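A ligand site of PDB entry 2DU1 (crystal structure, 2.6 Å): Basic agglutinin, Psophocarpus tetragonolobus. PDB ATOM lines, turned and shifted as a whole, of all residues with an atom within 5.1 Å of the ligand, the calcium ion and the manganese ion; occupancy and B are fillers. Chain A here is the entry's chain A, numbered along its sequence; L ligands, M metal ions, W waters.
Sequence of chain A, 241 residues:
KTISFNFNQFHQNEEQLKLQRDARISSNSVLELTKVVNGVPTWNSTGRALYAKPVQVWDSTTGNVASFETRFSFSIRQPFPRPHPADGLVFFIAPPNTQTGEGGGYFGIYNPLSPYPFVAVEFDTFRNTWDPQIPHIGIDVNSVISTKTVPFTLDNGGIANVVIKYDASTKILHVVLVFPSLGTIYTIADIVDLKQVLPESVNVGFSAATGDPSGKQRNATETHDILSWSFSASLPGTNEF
An oxygen (O5) of the ligand sits at hydrogen-bond distance from the side-chain amide nitrogen (ND2) of Asn 128 (3.1 Å).
An oxygen (O5) of the ligand is in hydrogen-bond range of the side-chain carboxylate (OD2) of Asp 87.
The backbone NH (N) of Gly 105 lies within hydrogen-bond range of an oxygen (O5) of the ligand.
An oxygen (O6) of the ligand lies within hydrogen-bond range of the backbone NH (N) of Asp 212 (3.0 Å).
OD1 of Asp 131 sits close to NE1 of Trp 130 (3.2 Å).
O of Asp 131 is in hydrogen-bond range of NE of Arg 127, 2.9 Å away.
The side-chain carboxylate (OD2) of Asp 87 lies within hydrogen-bond range of the backbone NH (N) of Gly 105.
OD1 of Asp 87 is in hydrogen-bond range of N of Gly 211.
OG of Ser 214 sits at hydrogen-bond distance from OD2 of Asp 212, at 2.8 Å.
N of Gly 211 sits at hydrogen-bond distance from O of Ala 220 (2.7 Å).
Residues that only touch the ligand: Gly 211 (3.3 Å), Gly 215 (3.4 Å), Gly 104 (3.4 Å), His 84 (3.6 Å), Ala 220 (3.6 Å) and Ser 214 (3.7 Å).
Of the 27 residues printed, 11 come within 4 Å of the ligand.
The nearest printed residue that does not touch the ligand is Ala 86 (4.02 Å).
Within 4 Å of the calcium ion: Asp 124, Phe 126, Asn 128 and Asp 131.
Within 4 Å of the manganese ion: Glu 122, Asp 124, Asp 131 and His 136.
The nearest printed residue that does not touch the manganese ion is Ser 146 (4.4 Å).
The calcium ion is bound by the side-chain carboxylate (OD1) of Asp 124, water W3, the backbone carbonyl oxygen (O) of Phe 126, the side-chain carboxylate (OD2) of Asp 131, the side-chain amide oxygen (OD1) of Asn 128 and the side-chain carboxylate (OD2) of Asp 124.
The calcium ion has six donor atoms within binding distance.
The manganese ion is bound by NE2 of His 136, at 2.3 Å.
Water W1 binds the manganese ion, at 2.3 Å.
OE2 of Glu 122 binds the manganese ion.
OD2 of Asp 124 is bound to the manganese ion, 2.3 Å away.
The manganese ion is bound by OD1 of Asp 131 (2.4 Å).
The manganese ion is bound by water W2 (2.4 Å).
Water W3 bridges O of Gly 105 (2.8 Å) and NE1 of Trp 130 (3.3 Å).
Water W1 lies within hydrogen-bond range of O of Val 144 (2.8 Å), OE1 of Glu 122 (2.9 Å) and NE1 of Trp 130 (3.3 Å).
Water W4 lies within hydrogen-bond range of OG of Ser 214 (3.3 Å) and N1 of the ligand (3.4 Å).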
ATOM      1  N   HIS A  84     -22.181 -27.701 -27.502  1.00  0.00           N
ATOM      2  CA  HIS A  84     -23.525 -27.813 -26.939  1.00  0.00           C
ATOM      3  C   HIS A  84     -24.448 -26.641 -27.297  1.00  0.00           C
ATOM      4  O   HIS A  84     -24.084 -25.473 -27.153  1.00  0.00           O
ATOM      5  CB  HIS A  84     -23.403 -27.912 -25.418  1.00  0.00           C
ATOM      6  CG  HIS A  84     -22.434 -26.918 -24.839  1.00  0.00           C
ATOM      7  ND1 HIS A  84     -21.241 -27.308 -24.250  1.00  0.00           N
ATOM      8  CD2 HIS A  84     -22.448 -25.564 -24.803  1.00  0.00           C
ATOM      9  CE1 HIS A  84     -20.577 -26.228 -23.883  1.00  0.00           C
ATOM     10  NE2 HIS A  84     -21.284 -25.166 -24.203  1.00  0.00           N
ATOM     11  N   ALA A  86     -27.687 -23.947 -27.044  1.00  0.00           N
ATOM     12  CA  ALA A  86     -28.213 -23.168 -25.924  1.00  0.00           C
ATOM     13  C   ALA A  86     -29.052 -22.010 -26.431  1.00  0.00           C
ATOM     14  O   ALA A  86     -28.836 -21.529 -27.534  1.00  0.00           O
ATOM     15  CB  ALA A  86     -27.046 -22.622 -25.081  1.00  0.00           C
ATOM     16  N   ASP A  87     -30.024 -21.561 -25.638  1.00  0.00           N
ATOM     17  CA  ASP A  87     -30.317 -22.124 -24.327  1.00  0.00           C
ATOM     18  C   ASP A  87     -31.711 -22.749 -24.268  1.00  0.00           C
ATOM     19  O   ASP A  87     -31.986 -23.614 -23.426  1.00  0.00           O
ATOM     20  CB  ASP A  87     -30.199 -21.038 -23.249  1.00  0.00           C
ATOM     21  CG  ASP A  87     -28.799 -20.922 -22.699  1.00  0.00           C
ATOM     22  OD1 ASP A  87     -27.981 -20.181 -23.312  1.00  0.00           O
ATOM     23  OD2 ASP A  87     -28.505 -21.566 -21.669  1.00  0.00           O
ATOM     24  N   GLY A 103     -29.937 -13.232 -19.805  1.00  0.00           N
ATOM     25  CA  GLY A 103     -29.969 -14.225 -20.869  1.00  0.00           C
ATOM     26  C   GLY A 103     -29.496 -15.579 -20.407  1.00  0.00           C
ATOM     27  O   GLY A 103     -29.733 -15.958 -19.256  1.00  0.00           O
ATOM     28  N   GLY A 104     -28.843 -16.320 -21.294  1.00  0.00           N
ATOM     29  CA  GLY A 104     -28.355 -17.647 -20.938  1.00  0.00           C
ATOM     30  C   GLY A 104     -29.428 -18.553 -20.352  1.00  0.00           C
ATOM     31  O   GLY A 104     -30.576 -18.545 -20.815  1.00  0.00           O
ATOM     32  N   GLY A 105     -29.056 -19.330 -19.343  1.00  0.00           N
ATOM     33  CA  GLY A 105     -29.981 -20.244 -18.716  1.00  0.00           C
ATOM     34  C   GLY A 105     -31.190 -19.615 -18.073  1.00  0.00           C
ATOM     35  O   GLY A 105     -32.076 -20.332 -17.619  1.00  0.00           O
ATOM     36  N   TYR A 106     -31.243 -18.284 -18.036  1.00  0.00           N
ATOM     37  CA  TYR A 106     -32.407 -17.605 -17.439  1.00  0.00           C
ATOM     38  C   TYR A 106     -33.443 -17.219 -18.482  1.00  0.00           C
ATOM     39  O   TYR A 106     -34.476 -16.644 -18.161  1.00  0.00           O
ATOM     40  CB  TYR A 106     -31.969 -16.379 -16.645  1.00  0.00           C
ATOM     41  CG  TYR A 106     -31.120 -16.727 -15.446  1.00  0.00           C
ATOM     42  CD1 TYR A 106     -31.647 -17.427 -14.368  1.00  0.00           C
ATOM     43  CD2 TYR A 106     -29.772 -16.390 -15.420  1.00  0.00           C
ATOM     44  CE1 TYR A 106     -30.839 -17.807 -13.290  1.00  0.00           C
ATOM     45  CE2 TYR A 106     -28.959 -16.756 -14.345  1.00  0.00           C
ATOM     46  CZ  TYR A 106     -29.501 -17.463 -13.283  1.00  0.00           C
ATOM     47  OH  TYR A 106     -28.682 -17.836 -12.231  1.00  0.00           O
ATOM     48  N   PHE A 107     -33.149 -17.542 -19.738  1.00  0.00           N
ATOM     49  CA  PHE A 107     -34.083 -17.320 -20.839  1.00  0.00           C
ATOM     50  C   PHE A 107     -34.534 -15.886 -21.058  1.00  0.00           C
ATOM     51  O   PHE A 107     -35.343 -15.622 -21.950  1.00  0.00           O
ATOM     52  CB  PHE A 107     -35.322 -18.192 -20.620  1.00  0.00           C
ATOM     53  CG  PHE A 107     -35.021 -19.639 -20.320  1.00  0.00           C
ATOM     54  CD1 PHE A 107     -34.502 -20.479 -21.300  1.00  0.00           C
ATOM     55  CD2 PHE A 107     -35.286 -20.177 -19.062  1.00  0.00           C
ATOM     56  CE1 PHE A 107     -34.260 -21.851 -21.040  1.00  0.00           C
ATOM     57  CE2 PHE A 107     -35.058 -21.541 -18.791  1.00  0.00           C
ATOM     58  CZ  PHE A 107     -34.549 -22.371 -19.772  1.00  0.00           C
ATOM     59  N   GLU A 122     -40.895 -24.204 -19.917  1.00  0.00           N
ATOM     60  CA  GLU A 122     -39.649 -24.152 -20.657  1.00  0.00           C
ATOM     61  C   GLU A 122     -39.345 -25.373 -21.515  1.00  0.00           C
ATOM     62  O   GLU A 122     -39.790 -26.485 -21.230  1.00  0.00           O
ATOM     63  CB  GLU A 122     -38.469 -23.970 -19.690  1.00  0.00           C
ATOM     64  CG  GLU A 122     -38.220 -25.208 -18.832  1.00  0.00           C
ATOM     65  CD  GLU A 122     -36.991 -25.096 -17.930  1.00  0.00           C
ATOM     66  OE1 GLU A 122     -36.869 -24.083 -17.210  1.00  0.00           O
ATOM     67  OE2 GLU A 122     -36.173 -26.033 -17.927  1.00  0.00           O
ATOM     68  N   ASP A 124     -35.959 -26.452 -22.399  1.00  0.00           N
ATOM     69  CA  ASP A 124     -34.559 -26.273 -22.071  1.00  0.00           C
ATOM     70  C   ASP A 124     -33.648 -27.152 -22.900  1.00  0.00           C
ATOM     71  O   ASP A 124     -33.796 -28.378 -22.898  1.00  0.00           O
ATOM     72  CB  ASP A 124     -34.378 -26.617 -20.590  1.00  0.00           C
ATOM     73  CG  ASP A 124     -33.177 -25.914 -19.971  1.00  0.00           C
ATOM     74  OD1 ASP A 124     -32.100 -25.868 -20.589  1.00  0.00           O
ATOM     75  OD2 ASP A 124     -33.330 -25.424 -18.842  1.00  0.00           O
ATOM     76  N   PHE A 126     -30.012 -26.552 -22.868  1.00  0.00           N
ATOM     77  CA  PHE A 126     -28.677 -26.541 -22.277  1.00  0.00           C
ATOM     78  C   PHE A 126     -28.741 -26.936 -20.815  1.00  0.00           C
ATOM     79  O   PHE A 126     -29.574 -26.431 -20.058  1.00  0.00           O
ATOM     80  CB  PHE A 126     -28.068 -25.142 -22.364  1.00  0.00           C
ATOM     81  CG  PHE A 126     -26.701 -25.067 -21.775  1.00  0.00           C
ATOM     82  CD1 PHE A 126     -25.592 -25.449 -22.523  1.00  0.00           C
ATOM     83  CD2 PHE A 126     -26.522 -24.659 -20.454  1.00  0.00           C
ATOM     84  CE1 PHE A 126     -24.306 -25.418 -21.957  1.00  0.00           C
ATOM     85  CE2 PHE A 126     -25.256 -24.627 -19.881  1.00  0.00           C
ATOM     86  CZ  PHE A 126     -24.148 -25.009 -20.629  1.00  0.00           C
ATOM     87  N   ARG A 127     -27.841 -27.814 -20.404  1.00  0.00           N
ATOM     88  CA  ARG A 127     -27.829 -28.267 -19.018  1.00  0.00           C
ATOM     89  C   ARG A 127     -27.035 -27.381 -18.075  1.00  0.00           C
ATOM     90  O   ARG A 127     -25.810 -27.429 -18.055  1.00  0.00           O
ATOM     91  CB  ARG A 127     -27.303 -29.702 -18.932  1.00  0.00           C
ATOM     92  CG  ARG A 127     -27.449 -30.287 -17.537  1.00  0.00           C
ATOM     93  CD  ARG A 127     -27.218 -31.783 -17.495  1.00  0.00           C
ATOM     94  NE  ARG A 127     -27.677 -32.313 -16.210  1.00  0.00           N
ATOM     95  CZ  ARG A 127     -27.541 -33.581 -15.822  1.00  0.00           C
ATOM     96  NH1 ARG A 127     -26.943 -34.460 -16.617  1.00  0.00           N
ATOM     97  NH2 ARG A 127     -28.011 -33.967 -14.634  1.00  0.00           N
ATOM     98  N   ASN A 128     -27.736 -26.571 -17.280  1.00  0.00           N
ATOM     99  CA  ASN A 128     -27.077 -25.719 -16.295  1.00  0.00           C
ATOM    100  C   ASN A 128     -26.869 -26.556 -15.049  1.00  0.00           C
ATOM    101  O   ASN A 128     -27.344 -27.685 -14.971  1.00  0.00           O
ATOM    102  CB  ASN A 128     -27.945 -24.490 -15.973  1.00  0.00           C
ATOM    103  CG  ASN A 128     -28.000 -23.458 -17.080  1.00  0.00           C
ATOM    104  OD1 ASN A 128     -28.890 -23.509 -17.934  1.00  0.00           O
ATOM    105  ND2 ASN A 128     -27.070 -22.518 -17.071  1.00  0.00           N
ATOM    106  N   TRP A 130     -28.249 -26.489 -12.326  1.00  0.00           N
ATOM    107  CA  TRP A 130     -29.523 -26.821 -11.698  1.00  0.00           C
ATOM    108  C   TRP A 130     -30.456 -27.658 -12.572  1.00  0.00           C
ATOM    109  O   TRP A 130     -31.599 -27.904 -12.190  1.00  0.00           O
ATOM    110  CB  TRP A 130     -30.244 -25.534 -11.312  1.00  0.00           C
ATOM    111  CG  TRP A 130     -30.541 -24.690 -12.501  1.00  0.00           C
ATOM    112  CD1 TRP A 130     -31.480 -24.937 -13.464  1.00  0.00           C
ATOM    113  CD2 TRP A 130     -29.846 -23.505 -12.918  1.00  0.00           C
ATOM    114  NE1 TRP A 130     -31.419 -23.986 -14.451  1.00  0.00           N
ATOM    115  CE2 TRP A 130     -30.419 -23.094 -14.138  1.00  0.00           C
ATOM    116  CE3 TRP A 130     -28.796 -22.753 -12.371  1.00  0.00           C
ATOM    117  CZ2 TRP A 130     -29.983 -21.953 -14.833  1.00  0.00           C
ATOM    118  CZ3 TRP A 130     -28.359 -21.619 -13.059  1.00  0.00           C
ATOM    119  CH2 TRP A 130     -28.949 -21.231 -14.267  1.00  0.00           C
ATOM    120  N   ASP A 131     -29.964 -28.090 -13.741  1.00  0.00           N
ATOM    121  CA  ASP A 131     -30.761 -28.876 -14.684  1.00  0.00           C
ATOM    122  C   ASP A 131     -30.511 -30.358 -14.734  1.00  0.00           C
ATOM    123  O   ASP A 131     -29.403 -30.825 -14.455  1.00  0.00           O
ATOM    124  CB  ASP A 131     -30.541 -28.422 -16.142  1.00  0.00           C
ATOM    125  CG  ASP A 131     -31.191 -27.107 -16.399  1.00  0.00           C
ATOM    126  OD1 ASP A 131     -32.208 -26.798 -15.731  1.00  0.00           O
ATOM    127  OD2 ASP A 131     -30.710 -26.395 -17.312  1.00  0.00           O
ATOM    128  N   PRO A 132     -31.543 -31.126 -15.103  1.00  0.00           N
ATOM    129  CA  PRO A 132     -31.434 -32.581 -15.232  1.00  0.00           C
ATOM    130  C   PRO A 132     -31.024 -32.713 -16.699  1.00  0.00           C
ATOM    131  O   PRO A 132     -30.810 -31.699 -17.365  1.00  0.00           O
ATOM    132  CB  PRO A 132     -32.858 -33.052 -14.959  1.00  0.00           C
ATOM    133  CG  PRO A 132     -33.690 -31.944 -15.475  1.00  0.00           C
ATOM    134  CD  PRO A 132     -32.952 -30.718 -14.967  1.00  0.00           C
ATOM    135  N   HIS A 136     -35.342 -30.924 -22.112  1.00  0.00           N
ATOM    136  CA  HIS A 136     -36.440 -31.279 -21.237  1.00  0.00           C
ATOM    137  C   HIS A 136     -37.473 -30.180 -21.170  1.00  0.00           C
ATOM    138  O   HIS A 136     -37.203 -29.013 -21.473  1.00  0.00           O
ATOM    139  CB  HIS A 136     -35.947 -31.629 -19.825  1.00  0.00           C
ATOM    140  CG  HIS A 136     -35.162 -30.552 -19.134  1.00  0.00           C
ATOM    141  ND1 HIS A 136     -33.797 -30.605 -18.997  1.00  0.00           N
ATOM    142  CD2 HIS A 136     -35.557 -29.398 -18.547  1.00  0.00           C
ATOM    143  CE1 HIS A 136     -33.373 -29.541 -18.344  1.00  0.00           C
ATOM    144  NE2 HIS A 136     -34.423 -28.790 -18.060  1.00  0.00           N
ATOM    145  N   VAL A 144     -36.098 -20.682 -12.393  1.00  0.00           N
ATOM    146  CA  VAL A 144     -35.791 -21.502 -13.541  1.00  0.00           C
ATOM    147  C   VAL A 144     -35.423 -22.902 -13.042  1.00  0.00           C
ATOM    148  O   VAL A 144     -34.955 -23.754 -13.793  1.00  0.00           O
ATOM    149  CB  VAL A 144     -34.631 -20.878 -14.339  1.00  0.00           C
ATOM    150  CG1 VAL A 144     -33.377 -20.807 -13.485  1.00  0.00           C
ATOM    151  CG2 VAL A 144     -34.400 -21.647 -15.605  1.00  0.00           C
ATOM    152  N   SER A 146     -37.073 -25.722 -12.241  1.00  0.00           N
ATOM    153  CA  SER A 146     -38.370 -26.374 -12.447  1.00  0.00           C
ATOM    154  C   SER A 146     -38.899 -27.196 -11.288  1.00  0.00           C
ATOM    155  O   SER A 146     -38.152 -27.875 -10.588  1.00  0.00           O
ATOM    156  CB  SER A 146     -38.293 -27.280 -13.680  1.00  0.00           C
ATOM    157  OG  SER A 146     -37.870 -26.544 -14.811  1.00  0.00           O
ATOM    158  N   THR A 210     -29.719 -17.520 -26.418  1.00  0.00           N
ATOM    159  CA  THR A 210     -28.671 -18.382 -26.952  1.00  0.00           C
ATOM    160  C   THR A 210     -27.510 -18.299 -25.977  1.00  0.00           C
ATOM    161  O   THR A 210     -27.568 -17.543 -24.995  1.00  0.00           O
ATOM    162  CB  THR A 210     -28.186 -17.939 -28.357  1.00  0.00           C
ATOM    163  OG1 THR A 210     -27.895 -16.527 -28.353  1.00  0.00           O
ATOM    164  CG2 THR A 210     -29.246 -18.226 -29.400  1.00  0.00           C
ATOM    165  N   GLY A 211     -26.462 -19.070 -26.251  1.00  0.00           N
ATOM    166  CA  GLY A 211     -25.296 -19.106 -25.366  1.00  0.00           C
ATOM    167  C   GLY A 211     -24.804 -17.778 -24.841  1.00  0.00           C
ATOM    168  O   GLY A 211     -24.727 -16.797 -25.576  1.00  0.00           O
ATOM    169  N   ASP A 212     -24.467 -17.737 -23.562  1.00  0.00           N
ATOM    170  CA  ASP A 212     -23.948 -16.522 -22.941  1.00  0.00           C
ATOM    171  C   ASP A 212     -22.440 -16.462 -23.197  1.00  0.00           C
ATOM    172  O   ASP A 212     -21.758 -17.499 -23.215  1.00  0.00           O
ATOM    173  CB  ASP A 212     -24.203 -16.523 -21.429  1.00  0.00           C
ATOM    174  CG  ASP A 212     -23.852 -15.195 -20.784  1.00  0.00           C
ATOM    175  OD1 ASP A 212     -24.762 -14.370 -20.562  1.00  0.00           O
ATOM    176  OD2 ASP A 212     -22.658 -14.963 -20.496  1.00  0.00           O
ATOM    177  N   SER A 214     -20.049 -15.765 -21.341  1.00  0.00           N
ATOM    178  CA  SER A 214     -19.298 -16.358 -20.245  1.00  0.00           C
ATOM    179  C   SER A 214     -18.952 -17.822 -20.485  1.00  0.00           C
ATOM    180  O   SER A 214     -18.042 -18.354 -19.867  1.00  0.00           O
ATOM    181  CB  SER A 214     -20.067 -16.214 -18.920  1.00  0.00           C
ATOM    182  OG  SER A 214     -21.303 -16.920 -18.937  1.00  0.00           O
ATOM    183  N   GLY A 215     -19.670 -18.463 -21.406  1.00  0.00           N
ATOM    184  CA  GLY A 215     -19.391 -19.862 -21.707  1.00  0.00           C
ATOM    185  C   GLY A 215     -18.257 -19.996 -22.701  1.00  0.00           C
ATOM    186  O   GLY A 215     -17.742 -21.092 -22.934  1.00  0.00           O
ATOM    187  N   LYS A 216     -17.875 -18.879 -23.306  1.00  0.00           N
ATOM    188  CA  LYS A 216     -16.810 -18.817 -24.291  1.00  0.00           C
ATOM    189  C   LYS A 216     -16.921 -19.840 -25.421  1.00  0.00           C
ATOM    190  O   LYS A 216     -15.929 -20.411 -25.870  1.00  0.00           O
ATOM    191  CB  LYS A 216     -15.449 -18.910 -23.595  1.00  0.00           C
ATOM    192  CG  LYS A 216     -15.136 -17.679 -22.736  1.00  0.00           C
ATOM    193  CD  LYS A 216     -13.794 -17.777 -22.026  1.00  0.00           C
ATOM    194  CE  LYS A 216     -13.456 -16.490 -21.261  1.00  0.00           C
ATOM    195  NZ  LYS A 216     -14.438 -16.177 -20.173  1.00  0.00           N
ATOM    196  N   GLN A 217     -18.163 -20.043 -25.882  1.00  0.00           N
ATOM    197  CA  GLN A 217     -18.454 -20.962 -26.981  1.00  0.00           C
ATOM    198  C   GLN A 217     -19.462 -20.305 -27.922  1.00  0.00           C
ATOM    199  O   GLN A 217     -20.633 -20.191 -27.592  1.00  0.00           O
ATOM    200  CB  GLN A 217     -19.002 -22.297 -26.462  1.00  0.00           C
ATOM    201  CG  GLN A 217     -18.005 -23.133 -25.664  1.00  0.00           C
ATOM    202  CD  GLN A 217     -16.754 -23.522 -26.453  1.00  0.00           C
ATOM    203  OE1 GLN A 217     -15.975 -22.654 -26.846  1.00  0.00           O
ATOM    204  NE2 GLN A 217     -16.566 -24.811 -26.681  1.00  0.00           N
ATOM    205  N   ALA A 220     -22.528 -22.296 -29.059  1.00  0.00           N
ATOM    206  CA  ALA A 220     -23.596 -22.484 -28.098  1.00  0.00           C
ATOM    207  C   ALA A 220     -24.794 -21.641 -28.540  1.00  0.00           C
ATOM    208  O   ALA A 220     -25.101 -20.615 -27.929  1.00  0.00           O
ATOM    209  CB  ALA A 220     -23.147 -22.064 -26.718  1.00  0.00           C
HETATM  210  O1  LIG L   1     -21.678 -21.739 -23.294  1.00  0.00           O
HETATM  211  C1  LIG L   1     -23.090 -21.612 -23.148  1.00  0.00           C
HETATM  212  C2  LIG L   1     -23.483 -21.494 -21.685  1.00  0.00           C
HETATM  213  O2  LIG L   1     -22.809 -20.331 -21.110  1.00  0.00           O
HETATM  214  C3  LIG L   1     -23.088 -20.128 -19.663  1.00  0.00           C
HETATM  215  O3  LIG L   1     -22.578 -21.162 -18.797  1.00  0.00           O
HETATM  216  C4  LIG L   1     -21.174 -21.450 -18.843  1.00  0.00           C
HETATM  217  C5  LIG L   1     -24.615 -19.969 -19.458  1.00  0.00           C
HETATM  218  N1  LIG L   1     -24.893 -19.786 -18.031  1.00  0.00           N
HETATM  219  C6  LIG L   1     -25.688 -18.806 -17.585  1.00  0.00           C
HETATM  220  O4  LIG L   1     -26.258 -17.990 -18.308  1.00  0.00           O
HETATM  221  C7  LIG L   1     -25.895 -18.746 -16.069  1.00  0.00           C
HETATM  222  C8  LIG L   1     -25.346 -21.215 -20.015  1.00  0.00           C
HETATM  223  O5  LIG L   1     -26.753 -21.095 -19.821  1.00  0.00           O
HETATM  224  C9  LIG L   1     -25.023 -21.361 -21.516  1.00  0.00           C
HETATM  225  O6  LIG L   1     -25.518 -20.220 -22.238  1.00  0.00           O
HETATM  226 CA    CA M   1     -30.873 -24.643 -19.038  1.00  0.00          CA
HETATM  227 MN    MN M   2     -34.137 -26.736 -17.085  1.00  0.00          MN
HETATM  228  O   HOH W   1     -34.130 -24.548 -16.337  1.00  0.00           O
HETATM  229  O   HOH W   2     -35.342 -27.141 -15.096  1.00  0.00           O
HETATM  230  O   HOH W   3     -31.963 -23.089 -17.547  1.00  0.00           O
HETATM  231  O   HOH W   4     -22.090 -18.824 -16.316  1.00  0.00           O
